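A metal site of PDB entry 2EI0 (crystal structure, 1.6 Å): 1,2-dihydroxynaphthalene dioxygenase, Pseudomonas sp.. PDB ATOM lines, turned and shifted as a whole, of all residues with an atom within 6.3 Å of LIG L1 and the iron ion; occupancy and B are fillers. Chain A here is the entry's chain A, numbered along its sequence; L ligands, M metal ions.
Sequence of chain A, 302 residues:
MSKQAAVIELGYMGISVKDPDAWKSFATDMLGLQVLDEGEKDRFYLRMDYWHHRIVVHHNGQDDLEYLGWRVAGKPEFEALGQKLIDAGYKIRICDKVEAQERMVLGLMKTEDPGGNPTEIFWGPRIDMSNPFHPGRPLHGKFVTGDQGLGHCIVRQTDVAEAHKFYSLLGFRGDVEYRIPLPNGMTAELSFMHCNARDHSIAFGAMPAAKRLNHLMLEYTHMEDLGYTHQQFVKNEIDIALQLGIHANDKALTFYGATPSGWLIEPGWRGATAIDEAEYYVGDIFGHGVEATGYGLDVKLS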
ATOM      1  N   HIS A 152     -13.860  13.037  20.079  1.00  0.00           N
ATOM      2  CA  HIS A 152     -14.745  12.252  20.946  1.00  0.00           C
ATOM      3  C   HIS A 152     -13.979  11.328  21.872  1.00  0.00           C
ATOM      4  O   HIS A 152     -12.838  10.970  21.587  1.00  0.00           O
ATOM      5  CB  HIS A 152     -15.842  11.492  20.170  1.00  0.00           C
ATOM      6  CG  HIS A 152     -15.367  10.314  19.359  1.00  0.00           C
ATOM      7  ND1 HIS A 152     -15.457  10.292  17.983  1.00  0.00           N
ATOM      8  CD2 HIS A 152     -14.911   9.090  19.724  1.00  0.00           C
ATOM      9  CE1 HIS A 152     -15.032   9.125  17.532  1.00  0.00           C
ATOM     10  NE2 HIS A 152     -14.710   8.368  18.568  1.00  0.00           N
ATOM     11  N   ILE A 154     -14.505   7.644  24.365  1.00  0.00           N
ATOM     12  CA  ILE A 154     -15.285   6.549  24.937  1.00  0.00           C
ATOM     13  C   ILE A 154     -14.768   6.405  26.359  1.00  0.00           C
ATOM     14  O   ILE A 154     -13.563   6.280  26.559  1.00  0.00           O
ATOM     15  CB  ILE A 154     -15.091   5.230  24.147  1.00  0.00           C
ATOM     16  CG1 ILE A 154     -15.960   5.199  22.888  1.00  0.00           C
ATOM     17  CG2 ILE A 154     -15.457   4.013  25.018  1.00  0.00           C
ATOM     18  CD1 ILE A 154     -15.917   6.451  21.988  1.00  0.00           C
ATOM     19  N   TYR A 178     -24.855   0.187  18.115  1.00  0.00           N
ATOM     20  CA  TYR A 178     -24.351  -1.107  17.666  1.00  0.00           C
ATOM     21  C   TYR A 178     -24.811  -2.208  18.574  1.00  0.00           C
ATOM     22  O   TYR A 178     -24.798  -2.040  19.798  1.00  0.00           O
ATOM     23  CB  TYR A 178     -22.830  -1.139  17.631  1.00  0.00           C
ATOM     24  CG  TYR A 178     -22.209  -0.327  16.511  1.00  0.00           C
ATOM     25  CD1 TYR A 178     -22.005   1.034  16.667  1.00  0.00           C
ATOM     26  CD2 TYR A 178     -21.831  -0.918  15.305  1.00  0.00           C
ATOM     27  CE1 TYR A 178     -21.432   1.811  15.671  1.00  0.00           C
ATOM     28  CE2 TYR A 178     -21.249  -0.130  14.279  1.00  0.00           C
ATOM     29  CZ  TYR A 178     -21.056   1.219  14.487  1.00  0.00           C
ATOM     30  OH  TYR A 178     -20.469   2.024  13.512  1.00  0.00           O
ATOM     31  N   ILE A 180     -23.522  -5.935  18.892  1.00  0.00           N
ATOM     32  CA  ILE A 180     -22.435  -6.778  18.397  1.00  0.00           C
ATOM     33  C   ILE A 180     -22.518  -8.188  18.995  1.00  0.00           C
ATOM     34  O   ILE A 180     -22.472  -8.334  20.221  1.00  0.00           O
ATOM     35  CB  ILE A 180     -21.046  -6.138  18.693  1.00  0.00           C
ATOM     36  CG1 ILE A 180     -20.934  -4.720  18.090  1.00  0.00           C
ATOM     37  CG2 ILE A 180     -19.918  -7.066  18.212  1.00  0.00           C
ATOM     38  CD1 ILE A 180     -21.185  -4.630  16.577  1.00  0.00           C
ATOM     39  N   LEU A 190     -23.615  -0.840  22.312  1.00  0.00           N
ATOM     40  CA  LEU A 190     -22.760   0.344  22.443  1.00  0.00           C
ATOM     41  C   LEU A 190     -23.573   1.581  22.134  1.00  0.00           C
ATOM     42  O   LEU A 190     -24.223   1.630  21.089  1.00  0.00           O
ATOM     43  CB  LEU A 190     -21.562   0.267  21.487  1.00  0.00           C
ATOM     44  CG  LEU A 190     -20.813  -1.075  21.467  1.00  0.00           C
ATOM     45  CD1 LEU A 190     -19.708  -1.028  20.418  1.00  0.00           C
ATOM     46  CD2 LEU A 190     -20.238  -1.429  22.815  1.00  0.00           C
ATOM     47  N   PHE A 192     -23.964   5.862  21.689  1.00  0.00           N
ATOM     48  CA  PHE A 192     -23.176   6.974  21.146  1.00  0.00           C
ATOM     49  C   PHE A 192     -24.017   8.230  21.201  1.00  0.00           C
ATOM     50  O   PHE A 192     -25.160   8.217  20.729  1.00  0.00           O
ATOM     51  CB  PHE A 192     -22.784   6.721  19.682  1.00  0.00           C
ATOM     52  CG  PHE A 192     -21.892   5.521  19.484  1.00  0.00           C
ATOM     53  CD1 PHE A 192     -22.436   4.226  19.479  1.00  0.00           C
ATOM     54  CD2 PHE A 192     -20.531   5.677  19.230  1.00  0.00           C
ATOM     55  CE1 PHE A 192     -21.618   3.112  19.282  1.00  0.00           C
ATOM     56  CE2 PHE A 192     -19.710   4.562  19.047  1.00  0.00           C
ATOM     57  CZ  PHE A 192     -20.263   3.286  19.060  1.00  0.00           C
ATOM     58  N   ASP A 199     -20.499  13.478  14.797  1.00  0.00           N
ATOM     59  CA  ASP A 199     -21.426  12.346  14.883  1.00  0.00           C
ATOM     60  C   ASP A 199     -21.594  11.851  16.323  1.00  0.00           C
ATOM     61  O   ASP A 199     -22.697  11.553  16.762  1.00  0.00           O
ATOM     62  CB  ASP A 199     -21.010  11.198  14.000  1.00  0.00           C
ATOM     63  CG  ASP A 199     -21.923  10.010  14.165  1.00  0.00           C
ATOM     64  OD1 ASP A 199     -23.002  10.013  13.521  1.00  0.00           O
ATOM     65  OD2 ASP A 199     -21.603   9.136  14.995  1.00  0.00           O
ATOM     66  N   HIS A 200     -20.488  11.739  17.053  1.00  0.00           N
ATOM     67  CA  HIS A 200     -20.581  11.539  18.487  1.00  0.00           C
ATOM     68  C   HIS A 200     -19.436  12.260  19.199  1.00  0.00           C
ATOM     69  O   HIS A 200     -18.358  12.439  18.610  1.00  0.00           O
ATOM     70  CB  HIS A 200     -20.637  10.059  18.899  1.00  0.00           C
ATOM     71  CG  HIS A 200     -19.594   9.190  18.245  1.00  0.00           C
ATOM     72  ND1 HIS A 200     -19.642   8.850  16.913  1.00  0.00           N
ATOM     73  CD2 HIS A 200     -18.509   8.551  18.762  1.00  0.00           C
ATOM     74  CE1 HIS A 200     -18.621   8.059  16.625  1.00  0.00           C
ATOM     75  NE2 HIS A 200     -17.926   7.863  17.721  1.00  0.00           N
ATOM     76  N   ASN A 214     -11.174   4.756  27.279  1.00  0.00           N
ATOM     77  CA  ASN A 214     -10.868   3.723  26.292  1.00  0.00           C
ATOM     78  C   ASN A 214     -10.090   4.305  25.126  1.00  0.00           C
ATOM     79  O   ASN A 214      -9.028   3.798  24.752  1.00  0.00           O
ATOM     80  CB  ASN A 214     -12.122   3.049  25.760  1.00  0.00           C
ATOM     81  CG  ASN A 214     -11.818   2.055  24.654  1.00  0.00           C
ATOM     82  OD1 ASN A 214     -12.000   2.349  23.461  1.00  0.00           O
ATOM     83  ND2 ASN A 214     -11.313   0.886  25.027  1.00  0.00           N
ATOM     84  N   HIS A 215     -10.636   5.361  24.534  1.00  0.00           N
ATOM     85  CA  HIS A 215      -9.944   6.045  23.446  1.00  0.00           C
ATOM     86  C   HIS A 215     -10.422   7.460  23.261  1.00  0.00           C
ATOM     87  O   HIS A 215     -11.527   7.817  23.676  1.00  0.00           O
ATOM     88  CB  HIS A 215     -10.013   5.265  22.104  1.00  0.00           C
ATOM     89  CG  HIS A 215     -11.322   5.341  21.385  1.00  0.00           C
ATOM     90  ND1 HIS A 215     -12.345   4.429  21.604  1.00  0.00           N
ATOM     91  CD2 HIS A 215     -11.766   6.164  20.403  1.00  0.00           C
ATOM     92  CE1 HIS A 215     -13.366   4.730  20.812  1.00  0.00           C
ATOM     93  NE2 HIS A 215     -13.032   5.769  20.071  1.00  0.00           N
ATOM     94  N   LEU A 216      -9.535   8.229  22.632  1.00  0.00           N
ATOM     95  CA  LEU A 216      -9.806   9.586  22.186  1.00  0.00           C
ATOM     96  C   LEU A 216      -9.658   9.586  20.666  1.00  0.00           C
ATOM     97  O   LEU A 216      -8.650   9.103  20.138  1.00  0.00           O
ATOM     98  CB  LEU A 216      -8.790  10.553  22.808  1.00  0.00           C
ATOM     99  CG  LEU A 216      -8.613  11.921  22.150  1.00  0.00           C
ATOM    100  CD1 LEU A 216      -9.903  12.750  22.325  1.00  0.00           C
ATOM    101  CD2 LEU A 216      -7.424  12.634  22.772  1.00  0.00           C
ATOM    102  N   MET A 217     -10.656  10.129  19.976  1.00  0.00           N
ATOM    103  CA  MET A 217     -10.597  10.291  18.532  1.00  0.00           C
ATOM    104  C   MET A 217     -10.274  11.748  18.184  1.00  0.00           C
ATOM    105  O   MET A 217     -10.918  12.667  18.691  1.00  0.00           O
ATOM    106  CB  MET A 217     -11.928   9.881  17.909  1.00  0.00           C
ATOM    107  CG  MET A 217     -11.952   9.804  16.383  1.00  0.00           C
ATOM    108  SD  MET A 217     -12.281  11.379  15.584  1.00  0.00           S
ATOM    109  CE  MET A 217     -12.015  10.839  13.891  1.00  0.00           C
ATOM    110  N   HIS A 247     -16.426   3.394  10.106  1.00  0.00           N
ATOM    111  CA  HIS A 247     -17.527   3.174  11.024  1.00  0.00           C
ATOM    112  C   HIS A 247     -18.856   3.311  10.329  1.00  0.00           C
ATOM    113  O   HIS A 247     -19.054   4.243   9.542  1.00  0.00           O
ATOM    114  CB  HIS A 247     -17.511   4.246  12.111  1.00  0.00           C
ATOM    115  CG  HIS A 247     -16.353   4.147  13.042  1.00  0.00           C
ATOM    116  ND1 HIS A 247     -16.053   2.994  13.723  1.00  0.00           N
ATOM    117  CD2 HIS A 247     -15.466   5.078  13.450  1.00  0.00           C
ATOM    118  CE1 HIS A 247     -15.011   3.205  14.502  1.00  0.00           C
ATOM    119  NE2 HIS A 247     -14.621   4.462  14.348  1.00  0.00           N
ATOM    120  N   ALA A 248     -19.799   2.424  10.670  1.00  0.00           N
ATOM    121  CA  ALA A 248     -21.158   2.524  10.110  1.00  0.00           C
ATOM    122  C   ALA A 248     -21.884   3.783  10.582  1.00  0.00           C
ATOM    123  O   ALA A 248     -22.634   4.384   9.815  1.00  0.00           O
ATOM    124  CB  ALA A 248     -21.976   1.268  10.429  1.00  0.00           C
ATOM    125  N   ASN A 249     -21.634   4.205  11.819  1.00  0.00           N
ATOM    126  CA  ASN A 249     -22.299   5.417  12.318  1.00  0.00           C
ATOM    127  C   ASN A 249     -21.745   6.749  11.772  1.00  0.00           C
ATOM    128  O   ASN A 249     -22.468   7.472  11.096  1.00  0.00           O
ATOM    129  CB  ASN A 249     -22.493   5.440  13.858  1.00  0.00           C
ATOM    130  CG  ASN A 249     -21.193   5.340  14.642  1.00  0.00           C
ATOM    131  OD1 ASN A 249     -20.087   5.373  14.092  1.00  0.00           O
ATOM    132  ND2 ASN A 249     -21.339   5.242  15.972  1.00  0.00           N
ATOM    133  N   ASP A 250     -20.465   7.057  12.028  1.00  0.00           N
ATOM    134  CA  ASP A 250     -19.953   8.354  11.596  1.00  0.00           C
ATOM    135  C   ASP A 250     -19.298   8.387  10.222  1.00  0.00           C
ATOM    136  O   ASP A 250     -18.933   9.467   9.739  1.00  0.00           O
ATOM    137  CB  ASP A 250     -19.064   9.011  12.641  1.00  0.00           C
ATOM    138  CG  ASP A 250     -17.693   8.366  12.783  1.00  0.00           C
ATOM    139  OD1 ASP A 250     -17.346   7.393  12.061  1.00  0.00           O
ATOM    140  OD2 ASP A 250     -16.948   8.855  13.650  1.00  0.00           O
ATOM    141  N   THR A 254     -10.761   5.617  10.013  1.00  0.00           N
ATOM    142  CA  THR A 254      -9.967   5.736  11.237  1.00  0.00           C
ATOM    143  C   THR A 254      -9.186   4.453  11.512  1.00  0.00           C
ATOM    144  O   THR A 254      -9.521   3.378  10.980  1.00  0.00           O
ATOM    145  CB  THR A 254     -10.847   6.000  12.495  1.00  0.00           C
ATOM    146  OG1 THR A 254     -11.366   4.750  12.983  1.00  0.00           O
ATOM    147  CG2 THR A 254     -12.021   6.980  12.236  1.00  0.00           C
ATOM    148  N   TYR A 256      -6.892   2.666  15.207  1.00  0.00           N
ATOM    149  CA  TYR A 256      -6.662   2.875  16.641  1.00  0.00           C
ATOM    150  C   TYR A 256      -5.251   2.443  17.003  1.00  0.00           C
ATOM    151  O   TYR A 256      -4.857   1.318  16.700  1.00  0.00           O
ATOM    152  CB  TYR A 256      -7.639   2.057  17.496  1.00  0.00           C
ATOM    153  CG  TYR A 256      -9.116   2.371  17.327  1.00  0.00           C
ATOM    154  CD1 TYR A 256      -9.792   2.120  16.118  1.00  0.00           C
ATOM    155  CD2 TYR A 256      -9.839   2.886  18.406  1.00  0.00           C
ATOM    156  CE1 TYR A 256     -11.145   2.402  15.992  1.00  0.00           C
ATOM    157  CE2 TYR A 256     -11.198   3.167  18.288  1.00  0.00           C
ATOM    158  CZ  TYR A 256     -11.844   2.904  17.085  1.00  0.00           C
ATOM    159  OH  TYR A 256     -13.192   3.173  16.986  1.00  0.00           O
ATOM    160  N   GLU A 266      -7.445   7.372  18.361  1.00  0.00           N
ATOM    161  CA  GLU A 266      -8.084   7.021  17.113  1.00  0.00           C
ATOM    162  C   GLU A 266      -7.946   8.191  16.142  1.00  0.00           C
ATOM    163  O   GLU A 266      -8.811   9.064  16.090  1.00  0.00           O
ATOM    164  CB  GLU A 266      -9.567   6.684  17.356  1.00  0.00           C
ATOM    165  CG  GLU A 266     -10.316   6.252  16.096  1.00  0.00           C
ATOM    166  CD  GLU A 266     -11.834   6.123  16.284  1.00  0.00           C
ATOM    167  OE1 GLU A 266     -12.373   6.545  17.336  1.00  0.00           O
ATOM    168  OE2 GLU A 266     -12.481   5.622  15.337  1.00  0.00           O
ATOM    169  N   GLY A 283     -22.329  -4.137  12.598  1.00  0.00           N
ATOM    170  CA  GLY A 283     -20.922  -4.177  12.216  1.00  0.00           C
ATOM    171  C   GLY A 283     -20.508  -2.949  11.423  1.00  0.00           C
ATOM    172  O   GLY A 283     -21.370  -2.144  11.016  1.00  0.00           O
ATOM    173  N   ASP A 284     -19.203  -2.803  11.217  1.00  0.00           N
ATOM    174  CA  ASP A 284     -18.711  -1.626  10.497  1.00  0.00           C
ATOM    175  C   ASP A 284     -18.760  -1.842   8.965  1.00  0.00           C
ATOM    176  O   ASP A 284     -19.120  -2.928   8.488  1.00  0.00           O
ATOM    177  CB  ASP A 284     -17.332  -1.193  11.032  1.00  0.00           C
ATOM    178  CG  ASP A 284     -17.448   0.007  12.014  1.00  0.00           C
ATOM    179  OD1 ASP A 284     -18.590   0.488  12.265  1.00  0.00           O
ATOM    180  OD2 ASP A 284     -16.401   0.487  12.516  1.00  0.00           O
ATOM    181  N   HIS A 288     -11.204  -2.178  10.440  1.00  0.00           N
ATOM    182  CA  HIS A 288     -11.210  -2.155  11.910  1.00  0.00           C
ATOM    183  C   HIS A 288     -11.023  -3.554  12.479  1.00  0.00           C
ATOM    184  O   HIS A 288     -11.605  -3.901  13.513  1.00  0.00           O
ATOM    185  CB  HIS A 288     -12.470  -1.494  12.456  1.00  0.00           C
ATOM    186  CG  HIS A 288     -12.477   0.004  12.314  1.00  0.00           C
ATOM    187  ND1 HIS A 288     -13.634   0.727  12.131  1.00  0.00           N
ATOM    188  CD2 HIS A 288     -11.467   0.901  12.336  1.00  0.00           C
ATOM    189  CE1 HIS A 288     -13.333   2.007  12.027  1.00  0.00           C
ATOM    190  NE2 HIS A 288     -12.032   2.151  12.163  1.00  0.00           N
HETATM  191  C1  LIG L   1     -17.376   2.230  16.865  1.00  0.00           C
HETATM  192  C2  LIG L   1     -16.288   2.609  17.641  1.00  0.00           C
HETATM  193  C3  LIG L   1     -15.884   3.921  17.698  1.00  0.00           C
HETATM  194  O1  LIG L   1     -14.801   4.230  18.469  1.00  0.00           O
HETATM  195  C4  LIG L   1     -16.553   4.905  16.967  1.00  0.00           C
HETATM  196  O2  LIG L   1     -16.102   6.203  17.042  1.00  0.00           O
HETATM  197  C5  LIG L   1     -17.658   4.549  16.168  1.00  0.00           C
HETATM  198  C6  LIG L   1     -18.062   3.206  16.122  1.00  0.00           C
HETATM  199  C7  LIG L   1     -17.695   0.779  16.835  1.00  0.00           C
HETATM  200  C8  LIG L   1     -17.466  -0.045  17.929  1.00  0.00           C
HETATM  201  C9  LIG L   1     -17.719  -1.418  17.849  1.00  0.00           C
HETATM  202  C10 LIG L   1     -18.189  -1.987  16.669  1.00  0.00           C
HETATM  203  C11 LIG L   1     -18.403  -1.173  15.549  1.00  0.00           C
HETATM  204  C12 LIG L   1     -18.128   0.198  15.632  1.00  0.00           C
HETATM  205  C1  LG2 L   2     -15.526   0.037  23.831  1.00  0.00           C
HETATM  206  C2  LG2 L   2     -15.206   0.214  25.192  1.00  0.00           C
HETATM  207  C3  LG2 L   2     -14.290  -0.631  25.823  1.00  0.00           C
HETATM  208  O1  LG2 L   2     -13.979  -0.461  27.142  1.00  0.00           O
HETATM  209  C4  LG2 L   2     -13.688  -1.652  25.085  1.00  0.00           C
HETATM  210  O2  LG2 L   2     -12.786  -2.484  25.684  1.00  0.00           O
HETATM  211  C5  LG2 L   2     -13.992  -1.841  23.734  1.00  0.00           C
HETATM  212  C6  LG2 L   2     -14.914  -0.996  23.112  1.00  0.00           C
HETATM  213  C7  LG2 L   2     -16.511   0.940  23.169  1.00  0.00           C
HETATM  214  C8  LG2 L   2     -17.667   1.322  23.873  1.00  0.00           C
HETATM  215  C9  LG2 L   2     -18.605   2.166  23.275  1.00  0.00           C
HETATM  216  C10 LG2 L   2     -18.409   2.630  21.972  1.00  0.00           C
HETATM  217  C11 LG2 L   2     -17.269   2.260  21.258  1.00  0.00           C
HETATM  218  C12 LG2 L   2     -16.323   1.415  21.861  1.00  0.00           C
HETATM  219 FE    FE M   1     -14.143   6.265  18.263  1.00  0.00          FE
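OH of Tyr 256 touches the iron ion, 3.5 Å away.
Four residues have an atom within 4 Å of the iron ion: His 152, His 215, Tyr 256 and Glu 266.
The side-chain carboxylate (OE1) of Glu 266 binds the iron ion, at 2.0 Å.
The iron ion is bound by an oxygen (O1) of LIG L1, at 2.1 Å.
NE2 of His 215 binds the iron ion (2.2 Å).
The iron ion is bound by a ring nitrogen (NE2) of His 152.
O2 of LIG L1 binds the iron ion, at 2.3 Å.
The iron ion has five donor atoms within binding distance.
A ring nitrogen (NE2) of His 200 lies close to an oxygen (O2) of LIG L1.
OH of Tyr 256 lies close to O1 of LIG L1, 2.4 Å away.
The side-chain carboxylate of Asp 284 is in hydrogen-bond range of the backbone NH of Ala 248.
The side-chain carboxylate (OD1) of Asp 284 is in hydrogen-bond range of the side-chain hydroxyl (OH) of Tyr 178 (2.7 Å).
The backbone carbonyl oxygen (O) of His 215 is in hydrogen-bond range of the backbone NH (N) of Ile 154.
The backbone NH (N) of Ala 248 lies within hydrogen-bond range of the side-chain hydroxyl (OH) of Tyr 178 (2.9 Å).
A ring nitrogen (ND1) of His 200 sits at hydrogen-bond distance from the side-chain carboxylate of Asp 199.
The side-chain carboxylate (OD2) of Asp 284 sits at hydrogen-bond distance from a ring nitrogen (ND1) of His 247, at 2.8 Å.
NE2 of His 247 sits close to OH of Tyr 256 (3.3 Å).
O of His 152 is in hydrogen-bond range of N of Met 217 (2.8 Å).
Tyr 178 touches LIG L1 (CE2 to C11, 3.3 Å).
Ile 180 touches LIG L1 (CD1 to C10, 3.996 Å).
Leu 190 touches LIG L1 (CD1 to C9, 3.3 Å).
CE2 of Phe 192 touches C5 of LIG L1, at 3.5 Å.
His 247 touches LIG L1.
Asn 249 touches LIG L1 (OD1 to C5, 3.3 Å).
OD1 of Asp 284 touches C12 of LIG L1 (3.4 Å).
Hydrophobic or aromatic side chains that line LIG L1: His 152, Tyr 178, Ile 180, Leu 190, Phe 192, His 200, His 215, His 247 and Tyr 256.
Within 4 Å of LIG L1: His 152, Tyr 178, Ile 180, Leu 190, Phe 192, His 200, His 215, His 247, Asn 249, Tyr 256, Glu 266 and Asp 284.
The nearest printed residue that does not touch LIG L1 is Ile 154 (4.3 Å).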
